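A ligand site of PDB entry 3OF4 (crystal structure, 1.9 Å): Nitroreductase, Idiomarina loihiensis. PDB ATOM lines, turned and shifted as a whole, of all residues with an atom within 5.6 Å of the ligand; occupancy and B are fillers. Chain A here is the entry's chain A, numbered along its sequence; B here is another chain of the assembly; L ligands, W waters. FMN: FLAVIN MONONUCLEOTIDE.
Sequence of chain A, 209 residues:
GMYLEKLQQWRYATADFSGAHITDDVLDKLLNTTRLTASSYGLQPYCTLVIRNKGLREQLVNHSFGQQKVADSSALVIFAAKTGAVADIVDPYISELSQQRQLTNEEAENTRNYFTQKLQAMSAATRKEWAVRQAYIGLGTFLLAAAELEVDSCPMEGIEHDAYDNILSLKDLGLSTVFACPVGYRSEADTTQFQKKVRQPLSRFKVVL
Water W1 lies within hydrogen-bond range of O of Ala 13 (2.8 Å), O2 of the ligand (3.2 Å) and SG of Cys 154 (3.6 Å).
Water W2 lies within hydrogen-bond range of the backbone NH of Val 198, an oxygen (O5') of the ligand and the guanidinium group of Arg 199.
The side-chain amide nitrogen (NE2) of Gln 67 is in hydrogen-bond range of the backbone carbonyl oxygen (O) of Gly 158 (2.9 Å).
The side-chain amino group of Lys 69 is in hydrogen-bond range of the side-chain amide oxygen of Gln 67 (3.4 Å).
The side-chain amino group (NZ) of Lys 197 is in hydrogen-bond range of the backbone carbonyl oxygen (O) of Arg 11.
The side-chain carboxylate (OE1) of Glu 157 sits at hydrogen-bond distance from the side-chain hydroxyl (OG) of Ser 40 of chain B (3.1 Å).
OE2 of Glu 157 sits at hydrogen-bond distance from NE2 of Gln 134 of chain B.
The side-chain hydroxyl (OH) of Tyr 136 sits at hydrogen-bond distance from the side-chain carboxylate (OE2) of Glu 157, at 2.6 Å.
The side-chain sulfur (SG) of Cys 154 sits close to the backbone carbonyl oxygen (O) of Thr 14 (3.7 Å).
The backbone NH (N) of Ser 40 of chain B sits at hydrogen-bond distance from the side-chain amide oxygen (OE1) of Gln 134 of chain B.
A nitrogen (N5) of the ligand lies close to the backbone carbonyl oxygen (O) of Pro 155.
Residues that only touch the ligand: Tyr 12 (3.4 Å), Met 156 (3.4 Å), Ser 39 of chain B (3.4 Å), Ala 38 of chain B (3.5 Å), Ile 137 of chain B (3.6 Å), Ser 40 of chain B (3.6 Å), Gln 134 of chain B (3.7 Å), Tyr 41 of chain B (3.9 Å) and Tyr 136 (3.9 Å).
Hydrophobic or aromatic side chains within 4 Å of the ligand: Tyr 12, Ala 13, Tyr 136, Pro 155, Met 156, Ala 38 of chain B and Ile 137 of chain B.
20 residues have an atom within 4 Å of the ligand: Arg 11, Tyr 12, Ala 13, Gln 67, Lys 69, Tyr 136, Cys 154, Pro 155, Met 156, Glu 157, Gly 158, Lys 197, Arg 199, Ala 38 of chain B, Ser 39 of chain B, Ser 40 of chain B, Tyr 41 of chain B, Gly 42 of chain B, Gln 134 of chain B and Ile 137 of chain B.
O2P of the ligand is in salt-bridge range of NH2 of Arg 199 (2.7 Å).
N3 of the ligand sits at hydrogen-bond distance from OE1 of Gln 67 (2.7 Å).
The backbone NH (N) of Ala 13 sits at hydrogen-bond distance from an oxygen (O3P) of the ligand.
An oxygen (O2P) of the ligand is in salt-bridge range of the side-chain amino group (NZ) of Lys 197, 2.9 Å away.
O4 of the ligand lies within hydrogen-bond range of N of Gly 158.
An oxygen (O1P) of the ligand is in salt-bridge range of the guanidinium group (NH2) of Arg 11 (3.1 Å).
A nitrogen (N5) of the ligand sits at hydrogen-bond distance from the backbone NH (N) of Glu 157 (3.2 Å).
NZ of Lys 69 is in hydrogen-bond range of O2 of the ligand.
An oxygen (O4') of the ligand sits at hydrogen-bond distance from the backbone NH of Gly 42 of chain B, at 3.5 Å.
A nitrogen (N1) of the ligand sits at hydrogen-bond distance from the side-chain sulfur (SG) of Cys 154 (3.6 Å).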
ATOM      1  N   ARG A  11      11.147 -21.974   7.532  1.00  0.00           N
ATOM      2  CA  ARG A  11      11.057 -21.707   8.956  1.00  0.00           C
ATOM      3  C   ARG A  11      11.777 -22.741   9.788  1.00  0.00           C
ATOM      4  O   ARG A  11      12.015 -23.853   9.332  1.00  0.00           O
ATOM      5  CB  ARG A  11       9.583 -21.623   9.410  1.00  0.00           C
ATOM      6  CG  ARG A  11       8.766 -22.902   9.253  1.00  0.00           C
ATOM      7  CD  ARG A  11       7.584 -22.928  10.200  1.00  0.00           C
ATOM      8  NE  ARG A  11       8.060 -22.802  11.574  1.00  0.00           N
ATOM      9  CZ  ARG A  11       8.693 -23.746  12.261  1.00  0.00           C
ATOM     10  NH1 ARG A  11       8.882 -24.973  11.789  1.00  0.00           N
ATOM     11  NH2 ARG A  11       9.118 -23.466  13.490  1.00  0.00           N
ATOM     12  N   TYR A  12      12.091 -22.358  11.020  1.00  0.00           N
ATOM     13  CA  TYR A  12      12.673 -23.315  11.996  1.00  0.00           C
ATOM     14  C   TYR A  12      12.441 -22.690  13.363  1.00  0.00           C
ATOM     15  O   TYR A  12      12.015 -21.516  13.478  1.00  0.00           O
ATOM     16  CB  TYR A  12      14.159 -23.621  11.718  1.00  0.00           C
ATOM     17  CG  TYR A  12      15.153 -22.562  12.167  1.00  0.00           C
ATOM     18  CD1 TYR A  12      15.184 -21.334  11.565  1.00  0.00           C
ATOM     19  CD2 TYR A  12      16.053 -22.806  13.205  1.00  0.00           C
ATOM     20  CE1 TYR A  12      16.084 -20.368  11.948  1.00  0.00           C
ATOM     21  CE2 TYR A  12      16.968 -21.826  13.619  1.00  0.00           C
ATOM     22  CZ  TYR A  12      16.974 -20.613  12.984  1.00  0.00           C
ATOM     23  OH  TYR A  12      17.876 -19.601  13.332  1.00  0.00           O
ATOM     24  N   ALA A  13      12.627 -23.496  14.395  1.00  0.00           N
ATOM     25  CA  ALA A  13      12.477 -23.026  15.770  1.00  0.00           C
ATOM     26  C   ALA A  13      13.774 -22.318  16.147  1.00  0.00           C
ATOM     27  O   ALA A  13      14.705 -22.922  16.625  1.00  0.00           O
ATOM     28  CB  ALA A  13      12.219 -24.212  16.718  1.00  0.00           C
ATOM     29  N   THR A  14      13.810 -21.023  15.886  1.00  0.00           N
ATOM     30  CA  THR A  14      14.998 -20.187  16.102  1.00  0.00           C
ATOM     31  C   THR A  14      15.572 -20.240  17.528  1.00  0.00           C
ATOM     32  O   THR A  14      14.875 -19.919  18.507  1.00  0.00           O
ATOM     33  CB  THR A  14      14.671 -18.755  15.750  1.00  0.00           C
ATOM     34  OG1 THR A  14      14.231 -18.717  14.387  1.00  0.00           O
ATOM     35  CG2 THR A  14      15.944 -17.840  15.901  1.00  0.00           C
ATOM     36  N   GLN A  67      15.662 -19.677  29.098  1.00  0.00           N
ATOM     37  CA  GLN A  67      15.734 -19.564  27.655  1.00  0.00           C
ATOM     38  C   GLN A  67      15.825 -18.072  27.322  1.00  0.00           C
ATOM     39  O   GLN A  67      14.835 -17.360  27.323  1.00  0.00           O
ATOM     40  CB  GLN A  67      14.513 -20.235  27.021  1.00  0.00           C
ATOM     41  CG  GLN A  67      14.531 -21.721  27.157  1.00  0.00           C
ATOM     42  CD  GLN A  67      13.330 -22.381  26.515  1.00  0.00           C
ATOM     43  OE1 GLN A  67      13.412 -22.800  25.369  1.00  0.00           O
ATOM     44  NE2 GLN A  67      12.217 -22.477  27.236  1.00  0.00           N
ATOM     45  N   LYS A  69      16.246 -16.503  24.582  1.00  0.00           N
ATOM     46  CA  LYS A  69      15.539 -16.035  23.350  1.00  0.00           C
ATOM     47  C   LYS A  69      14.273 -15.180  23.629  1.00  0.00           C
ATOM     48  O   LYS A  69      13.897 -14.332  22.828  1.00  0.00           O
ATOM     49  CB  LYS A  69      15.204 -17.223  22.426  1.00  0.00           C
ATOM     50  CG  LYS A  69      14.415 -18.333  23.081  1.00  0.00           C
ATOM     51  CD  LYS A  69      13.864 -19.409  22.113  1.00  0.00           C
ATOM     52  CE  LYS A  69      14.872 -20.535  21.809  1.00  0.00           C
ATOM     53  NZ  LYS A  69      15.334 -21.231  23.036  1.00  0.00           N
ATOM     54  N   TYR A 136      -3.946 -22.847  19.479  1.00  0.00           N
ATOM     55  CA  TYR A 136      -2.974 -23.695  18.787  1.00  0.00           C
ATOM     56  C   TYR A 136      -3.229 -23.719  17.296  1.00  0.00           C
ATOM     57  O   TYR A 136      -2.292 -23.711  16.515  1.00  0.00           O
ATOM     58  CB  TYR A 136      -2.979 -25.132  19.392  1.00  0.00           C
ATOM     59  CG  TYR A 136      -2.102 -25.240  20.586  1.00  0.00           C
ATOM     60  CD1 TYR A 136      -0.743 -25.490  20.446  1.00  0.00           C
ATOM     61  CD2 TYR A 136      -2.601 -25.094  21.887  1.00  0.00           C
ATOM     62  CE1 TYR A 136       0.092 -25.540  21.546  1.00  0.00           C
ATOM     63  CE2 TYR A 136      -1.765 -25.173  23.001  1.00  0.00           C
ATOM     64  CZ  TYR A 136      -0.412 -25.387  22.815  1.00  0.00           C
ATOM     65  OH  TYR A 136       0.458 -25.512  23.858  1.00  0.00           O
ATOM     66  N   LEU A 139      -1.575 -20.619  16.156  1.00  0.00           N
ATOM     67  CA  LEU A 139      -0.114 -20.827  16.058  1.00  0.00           C
ATOM     68  C   LEU A 139       0.299 -21.439  14.697  1.00  0.00           C
ATOM     69  O   LEU A 139       1.319 -21.044  14.096  1.00  0.00           O
ATOM     70  CB  LEU A 139       0.400 -21.723  17.180  1.00  0.00           C
ATOM     71  CG  LEU A 139       1.893 -22.056  17.211  1.00  0.00           C
ATOM     72  CD1 LEU A 139       2.726 -20.759  17.246  1.00  0.00           C
ATOM     73  CD2 LEU A 139       2.156 -22.954  18.457  1.00  0.00           C
ATOM     74  N   LEU A 143       3.015 -19.425  12.374  1.00  0.00           N
ATOM     75  CA  LEU A 143       4.298 -19.981  11.956  1.00  0.00           C
ATOM     76  C   LEU A 143       4.512 -19.837  10.430  1.00  0.00           C
ATOM     77  O   LEU A 143       5.589 -19.422   9.989  1.00  0.00           O
ATOM     78  CB  LEU A 143       4.447 -21.433  12.424  1.00  0.00           C
ATOM     79  CG  LEU A 143       4.563 -21.655  13.958  1.00  0.00           C
ATOM     80  CD1 LEU A 143       4.544 -23.151  14.212  1.00  0.00           C
ATOM     81  CD2 LEU A 143       5.813 -20.973  14.595  1.00  0.00           C
ATOM     82  N   CYS A 154      10.101 -18.654  17.388  1.00  0.00           N
ATOM     83  CA  CYS A 154      10.208 -19.938  18.047  1.00  0.00           C
ATOM     84  C   CYS A 154       9.010 -20.060  18.950  1.00  0.00           C
ATOM     85  O   CYS A 154       8.795 -19.226  19.812  1.00  0.00           O
ATOM     86  CB  CYS A 154      11.487 -20.051  18.857  1.00  0.00           C
ATOM     87  SG  CYS A 154      11.796 -21.666  19.497  1.00  0.00           S
ATOM     88  N   PRO A 155       8.150 -21.028  18.706  1.00  0.00           N
ATOM     89  CA  PRO A 155       7.053 -21.278  19.677  1.00  0.00           C
ATOM     90  C   PRO A 155       7.635 -21.808  20.968  1.00  0.00           C
ATOM     91  O   PRO A 155       8.622 -22.506  20.914  1.00  0.00           O
ATOM     92  CB  PRO A 155       6.257 -22.407  19.022  1.00  0.00           C
ATOM     93  CG  PRO A 155       6.908 -22.704  17.729  1.00  0.00           C
ATOM     94  CD  PRO A 155       8.253 -22.068  17.684  1.00  0.00           C
ATOM     95  N   MET A 156       6.979 -21.539  22.101  1.00  0.00           N
ATOM     96  CA  MET A 156       7.546 -21.843  23.438  1.00  0.00           C
ATOM     97  C   MET A 156       6.448 -22.223  24.422  1.00  0.00           C
ATOM     98  O   MET A 156       5.612 -21.379  24.810  1.00  0.00           O
ATOM     99  CB  MET A 156       8.350 -20.662  24.009  1.00  0.00           C
ATOM    100  CG  MET A 156       9.599 -20.306  23.192  1.00  0.00           C
ATOM    101  SD  MET A 156      10.484 -18.821  24.011  1.00  0.00           S
ATOM    102  CE  MET A 156      11.078 -19.703  25.683  1.00  0.00           C
ATOM    103  N   GLU A 157       6.458 -23.514  24.782  1.00  0.00           N
ATOM    104  CA  GLU A 157       5.645 -24.087  25.859  1.00  0.00           C
ATOM    105  C   GLU A 157       6.486 -24.251  27.114  1.00  0.00           C
ATOM    106  O   GLU A 157       5.938 -24.426  28.174  1.00  0.00           O
ATOM    107  CB  GLU A 157       5.147 -25.501  25.471  1.00  0.00           C
ATOM    108  CG  GLU A 157       3.796 -25.598  24.711  1.00  0.00           C
ATOM    109  CD  GLU A 157       3.464 -27.047  24.179  1.00  0.00           C
ATOM    110  OE1 GLU A 157       4.393 -27.924  24.276  1.00  0.00           O
ATOM    111  OE2 GLU A 157       2.289 -27.287  23.683  1.00  0.00           O
ATOM    112  N   GLY A 158       7.810 -24.219  26.992  1.00  0.00           N
ATOM    113  CA  GLY A 158       8.663 -24.371  28.166  1.00  0.00           C
ATOM    114  C   GLY A 158       8.787 -23.080  28.956  1.00  0.00           C
ATOM    115  O   GLY A 158       9.882 -22.458  29.025  1.00  0.00           O
ATOM    116  N   ILE A 159       7.659 -22.671  29.503  1.00  0.00           N
ATOM    117  CA  ILE A 159       7.567 -21.474  30.298  1.00  0.00           C
ATOM    118  C   ILE A 159       6.771 -21.836  31.551  1.00  0.00           C
ATOM    119  O   ILE A 159       5.990 -22.805  31.533  1.00  0.00           O
ATOM    120  CB  ILE A 159       6.871 -20.333  29.511  1.00  0.00           C
ATOM    121  CG1 ILE A 159       5.462 -20.711  29.094  1.00  0.00           C
ATOM    122  CG2 ILE A 159       7.684 -19.912  28.245  1.00  0.00           C
ATOM    123  CD1 ILE A 159       4.723 -19.589  28.342  1.00  0.00           C
ATOM    124  N   PHE A 179       1.147 -20.072  25.219  1.00  0.00           N
ATOM    125  CA  PHE A 179       2.538 -20.227  24.810  1.00  0.00           C
ATOM    126  C   PHE A 179       3.043 -18.862  24.361  1.00  0.00           C
ATOM    127  O   PHE A 179       2.254 -17.974  24.000  1.00  0.00           O
ATOM    128  CB  PHE A 179       2.689 -21.276  23.674  1.00  0.00           C
ATOM    129  CG  PHE A 179       1.665 -21.166  22.589  1.00  0.00           C
ATOM    130  CD1 PHE A 179       1.816 -20.268  21.560  1.00  0.00           C
ATOM    131  CD2 PHE A 179       0.508 -21.954  22.607  1.00  0.00           C
ATOM    132  CE1 PHE A 179       0.830 -20.157  20.552  1.00  0.00           C
ATOM    133  CE2 PHE A 179      -0.458 -21.850  21.613  1.00  0.00           C
ATOM    134  CZ  PHE A 179      -0.325 -20.939  20.631  1.00  0.00           C
ATOM    135  N   LYS A 197      16.052 -30.657   8.848  1.00  0.00           N
ATOM    136  CA  LYS A 197      14.770 -30.661   9.493  1.00  0.00           C
ATOM    137  C   LYS A 197      14.288 -32.115   9.568  1.00  0.00           C
ATOM    138  O   LYS A 197      14.439 -32.882   8.618  1.00  0.00           O
ATOM    139  CB  LYS A 197      13.833 -29.686   8.714  1.00  0.00           C
ATOM    140  CG  LYS A 197      12.527 -29.380   9.355  1.00  0.00           C
ATOM    141  CD  LYS A 197      11.683 -28.326   8.594  1.00  0.00           C
ATOM    142  CE  LYS A 197      12.312 -26.926   8.587  1.00  0.00           C
ATOM    143  NZ  LYS A 197      12.756 -26.453   9.922  1.00  0.00           N
ATOM    144  N   VAL A 198      13.791 -32.506  10.738  1.00  0.00           N
ATOM    145  CA  VAL A 198      13.288 -33.848  11.033  1.00  0.00           C
ATOM    146  C   VAL A 198      11.761 -33.892  11.166  1.00  0.00           C
ATOM    147  O   VAL A 198      11.164 -33.206  12.013  1.00  0.00           O
ATOM    148  CB  VAL A 198      13.872 -34.344  12.361  1.00  0.00           C
ATOM    149  CG1 VAL A 198      13.437 -35.782  12.656  1.00  0.00           C
ATOM    150  CG2 VAL A 198      15.401 -34.259  12.327  1.00  0.00           C
ATOM    151  N   ARG A 199      11.131 -34.699  10.312  1.00  0.00           N
ATOM    152  CA  ARG A 199       9.703 -34.938  10.356  1.00  0.00           C
ATOM    153  C   ARG A 199       9.451 -36.370  10.028  1.00  0.00           C
ATOM    154  O   ARG A 199      10.178 -36.955   9.202  1.00  0.00           O
ATOM    155  CB  ARG A 199       8.976 -34.068   9.316  1.00  0.00           C
ATOM    156  CG  ARG A 199       9.097 -32.604   9.549  1.00  0.00           C
ATOM    157  CD  ARG A 199       8.389 -32.115  10.784  1.00  0.00           C
ATOM    158  NE  ARG A 199       8.327 -30.655  10.817  1.00  0.00           N
ATOM    159  CZ  ARG A 199       9.261 -29.854  11.333  1.00  0.00           C
ATOM    160  NH1 ARG A 199      10.339 -30.346  11.924  1.00  0.00           N
ATOM    161  NH2 ARG A 199       9.092 -28.540  11.281  1.00  0.00           N
ATOM    162  N   ALA B  38       5.465 -27.765  12.624  1.00  0.00           N
ATOM    163  CA  ALA B  38       6.182 -27.815  13.900  1.00  0.00           C
ATOM    164  C   ALA B  38       5.320 -28.429  14.994  1.00  0.00           C
ATOM    165  O   ALA B  38       4.075 -28.220  15.065  1.00  0.00           O
ATOM    166  CB  ALA B  38       6.613 -26.410  14.339  1.00  0.00           C
ATOM    167  N   SER B  39       6.004 -29.136  15.890  1.00  0.00           N
ATOM    168  CA  SER B  39       5.372 -29.728  17.059  1.00  0.00           C
ATOM    169  C   SER B  39       6.298 -29.672  18.245  1.00  0.00           C
ATOM    170  O   SER B  39       7.505 -29.511  18.082  1.00  0.00           O
ATOM    171  CB  SER B  39       5.011 -31.190  16.798  1.00  0.00           C
ATOM    172  OG  SER B  39       6.156 -31.938  16.459  1.00  0.00           O
ATOM    173  N   SER B  40       5.704 -29.757  19.421  1.00  0.00           N
ATOM    174  CA  SER B  40       6.466 -29.825  20.685  1.00  0.00           C
ATOM    175  C   SER B  40       7.541 -30.898  20.651  1.00  0.00           C
ATOM    176  O   SER B  40       7.260 -32.062  20.302  1.00  0.00           O
ATOM    177  CB  SER B  40       5.479 -30.046  21.854  1.00  0.00           C
ATOM    178  OG  SER B  40       6.161 -30.213  23.094  1.00  0.00           O
ATOM    179  N   TYR B  41       8.781 -30.483  20.956  1.00  0.00           N
ATOM    180  CA  TYR B  41       9.991 -31.307  20.899  1.00  0.00           C
ATOM    181  C   TYR B  41      10.215 -32.000  19.557  1.00  0.00           C
ATOM    182  O   TYR B  41      11.063 -32.884  19.449  1.00  0.00           O
ATOM    183  CB  TYR B  41       9.990 -32.321  22.074  1.00  0.00           C
ATOM    184  CG  TYR B  41      10.297 -31.674  23.421  1.00  0.00           C
ATOM    185  CD1 TYR B  41      11.587 -31.208  23.699  1.00  0.00           C
ATOM    186  CD2 TYR B  41       9.317 -31.502  24.401  1.00  0.00           C
ATOM    187  CE1 TYR B  41      11.906 -30.604  24.921  1.00  0.00           C
ATOM    188  CE2 TYR B  41       9.621 -30.887  25.640  1.00  0.00           C
ATOM    189  CZ  TYR B  41      10.917 -30.434  25.889  1.00  0.00           C
ATOM    190  OH  TYR B  41      11.279 -29.819  27.086  1.00  0.00           O
ATOM    191  N   GLY B  42       9.452 -31.604  18.536  1.00  0.00           N
ATOM    192  CA  GLY B  42       9.476 -32.275  17.232  1.00  0.00           C
ATOM    193  C   GLY B  42       8.829 -33.678  17.226  1.00  0.00           C
ATOM    194  O   GLY B  42       8.961 -34.428  16.261  1.00  0.00           O
ATOM    195  N   TYR B  93      10.240 -41.049  15.950  1.00  0.00           N
ATOM    196  CA  TYR B  93      11.008 -39.805  15.909  1.00  0.00           C
ATOM    197  C   TYR B  93      12.512 -40.074  15.965  1.00  0.00           C
ATOM    198  O   TYR B  93      13.270 -39.548  15.148  1.00  0.00           O
ATOM    199  CB  TYR B  93      10.599 -38.919  17.091  1.00  0.00           C
ATOM    200  CG  TYR B  93      11.487 -37.712  17.286  1.00  0.00           C
ATOM    201  CD1 TYR B  93      11.407 -36.650  16.429  1.00  0.00           C
ATOM    202  CD2 TYR B  93      12.417 -37.664  18.311  1.00  0.00           C
ATOM    203  CE1 TYR B  93      12.209 -35.554  16.580  1.00  0.00           C
ATOM    204  CE2 TYR B  93      13.217 -36.576  18.483  1.00  0.00           C
ATOM    205  CZ  TYR B  93      13.110 -35.518  17.602  1.00  0.00           C
ATOM    206  OH  TYR B  93      13.901 -34.413  17.750  1.00  0.00           O
ATOM    207  N   GLN B 134      -0.908 -30.401  19.847  1.00  0.00           N
ATOM    208  CA  GLN B 134      -0.012 -30.448  18.679  1.00  0.00           C
ATOM    209  C   GLN B 134      -0.828 -30.649  17.382  1.00  0.00           C
ATOM    210  O   GLN B 134      -0.555 -30.015  16.357  1.00  0.00           O
ATOM    211  CB  GLN B 134       1.022 -31.547  18.804  1.00  0.00           C
ATOM    212  CG  GLN B 134       1.886 -31.498  20.062  1.00  0.00           C
ATOM    213  CD  GLN B 134       2.220 -30.095  20.538  1.00  0.00           C
ATOM    214  OE1 GLN B 134       2.870 -29.312  19.831  1.00  0.00           O
ATOM    215  NE2 GLN B 134       1.809 -29.778  21.775  1.00  0.00           N
ATOM    216  N   ILE B 137      -2.293 -27.441  15.940  1.00  0.00           N
ATOM    217  CA  ILE B 137      -1.341 -26.689  15.131  1.00  0.00           C
ATOM    218  C   ILE B 137      -1.366 -27.184  13.721  1.00  0.00           C
ATOM    219  O   ILE B 137      -1.366 -26.410  12.752  1.00  0.00           O
ATOM    220  CB  ILE B 137       0.171 -26.768  15.648  1.00  0.00           C
ATOM    221  CG1 ILE B 137       0.268 -26.536  17.197  1.00  0.00           C
ATOM    222  CG2 ILE B 137       1.034 -25.810  14.847  1.00  0.00           C
ATOM    223  CD1 ILE B 137       1.706 -26.666  17.758  1.00  0.00           C
HETATM  224  N1  FMN L   1      11.626 -24.705  21.340  1.00  0.00           N
HETATM  225  C2  FMN L   1      12.319 -24.118  22.367  1.00  0.00           C
HETATM  226  O2  FMN L   1      13.516 -23.806  22.198  1.00  0.00           O
HETATM  227  N3  FMN L   1      11.684 -23.869  23.576  1.00  0.00           N
HETATM  228  C4  FMN L   1      10.355 -24.206  23.768  1.00  0.00           C
HETATM  229  O4  FMN L   1       9.819 -23.963  24.860  1.00  0.00           O
HETATM  230  C4A FMN L   1       9.657 -24.807  22.711  1.00  0.00           C
HETATM  231  N5  FMN L   1       8.328 -25.172  22.844  1.00  0.00           N
HETATM  232  C5A FMN L   1       7.589 -25.482  21.701  1.00  0.00           C
HETATM  233  C6  FMN L   1       6.184 -25.555  21.774  1.00  0.00           C
HETATM  234  C7  FMN L   1       5.412 -25.856  20.646  1.00  0.00           C
HETATM  235  C7M FMN L   1       3.904 -25.924  20.733  1.00  0.00           C
HETATM  236  C8  FMN L   1       6.047 -26.076  19.424  1.00  0.00           C
HETATM  237  C8M FMN L   1       5.233 -26.412  18.181  1.00  0.00           C
HETATM  238  C9  FMN L   1       7.442 -26.014  19.351  1.00  0.00           C
HETATM  239  C9A FMN L   1       8.234 -25.711  20.482  1.00  0.00           C
HETATM  240  N10 FMN L   1       9.636 -25.646  20.430  1.00  0.00           N
HETATM  241  C10 FMN L   1      10.303 -25.057  21.493  1.00  0.00           C
HETATM  242  C1' FMN L   1      10.351 -25.821  19.114  1.00  0.00           C
HETATM  243  C2' FMN L   1      10.339 -27.268  18.683  1.00  0.00           C
HETATM  244  O2' FMN L   1      11.338 -27.912  19.408  1.00  0.00           O
HETATM  245  C3' FMN L   1      10.517 -27.391  17.136  1.00  0.00           C
HETATM  246  O3' FMN L   1       9.388 -26.836  16.510  1.00  0.00           O
HETATM  247  C4' FMN L   1      10.605 -28.829  16.638  1.00  0.00           C
HETATM  248  O4' FMN L   1      11.777 -29.401  17.180  1.00  0.00           O
HETATM  249  C5' FMN L   1      10.543 -28.988  15.088  1.00  0.00           C
HETATM  250  O5' FMN L   1      11.636 -28.364  14.415  1.00  0.00           O
HETATM  251  P   FMN L   1      11.524 -26.933  13.640  1.00  0.00           P
HETATM  252  O1P FMN L   1      10.436 -26.112  14.245  1.00  0.00           O
HETATM  253  O2P FMN L   1      11.234 -27.273  12.224  1.00  0.00           O
HETATM  254  O3P FMN L   1      12.848 -26.229  13.768  1.00  0.00           O
HETATM  255  O   HOH W   1      14.849 -23.585  19.304  1.00  0.00           O
HETATM  256  O   HOH W   2      13.531 -30.550  12.806  1.00  0.00           O
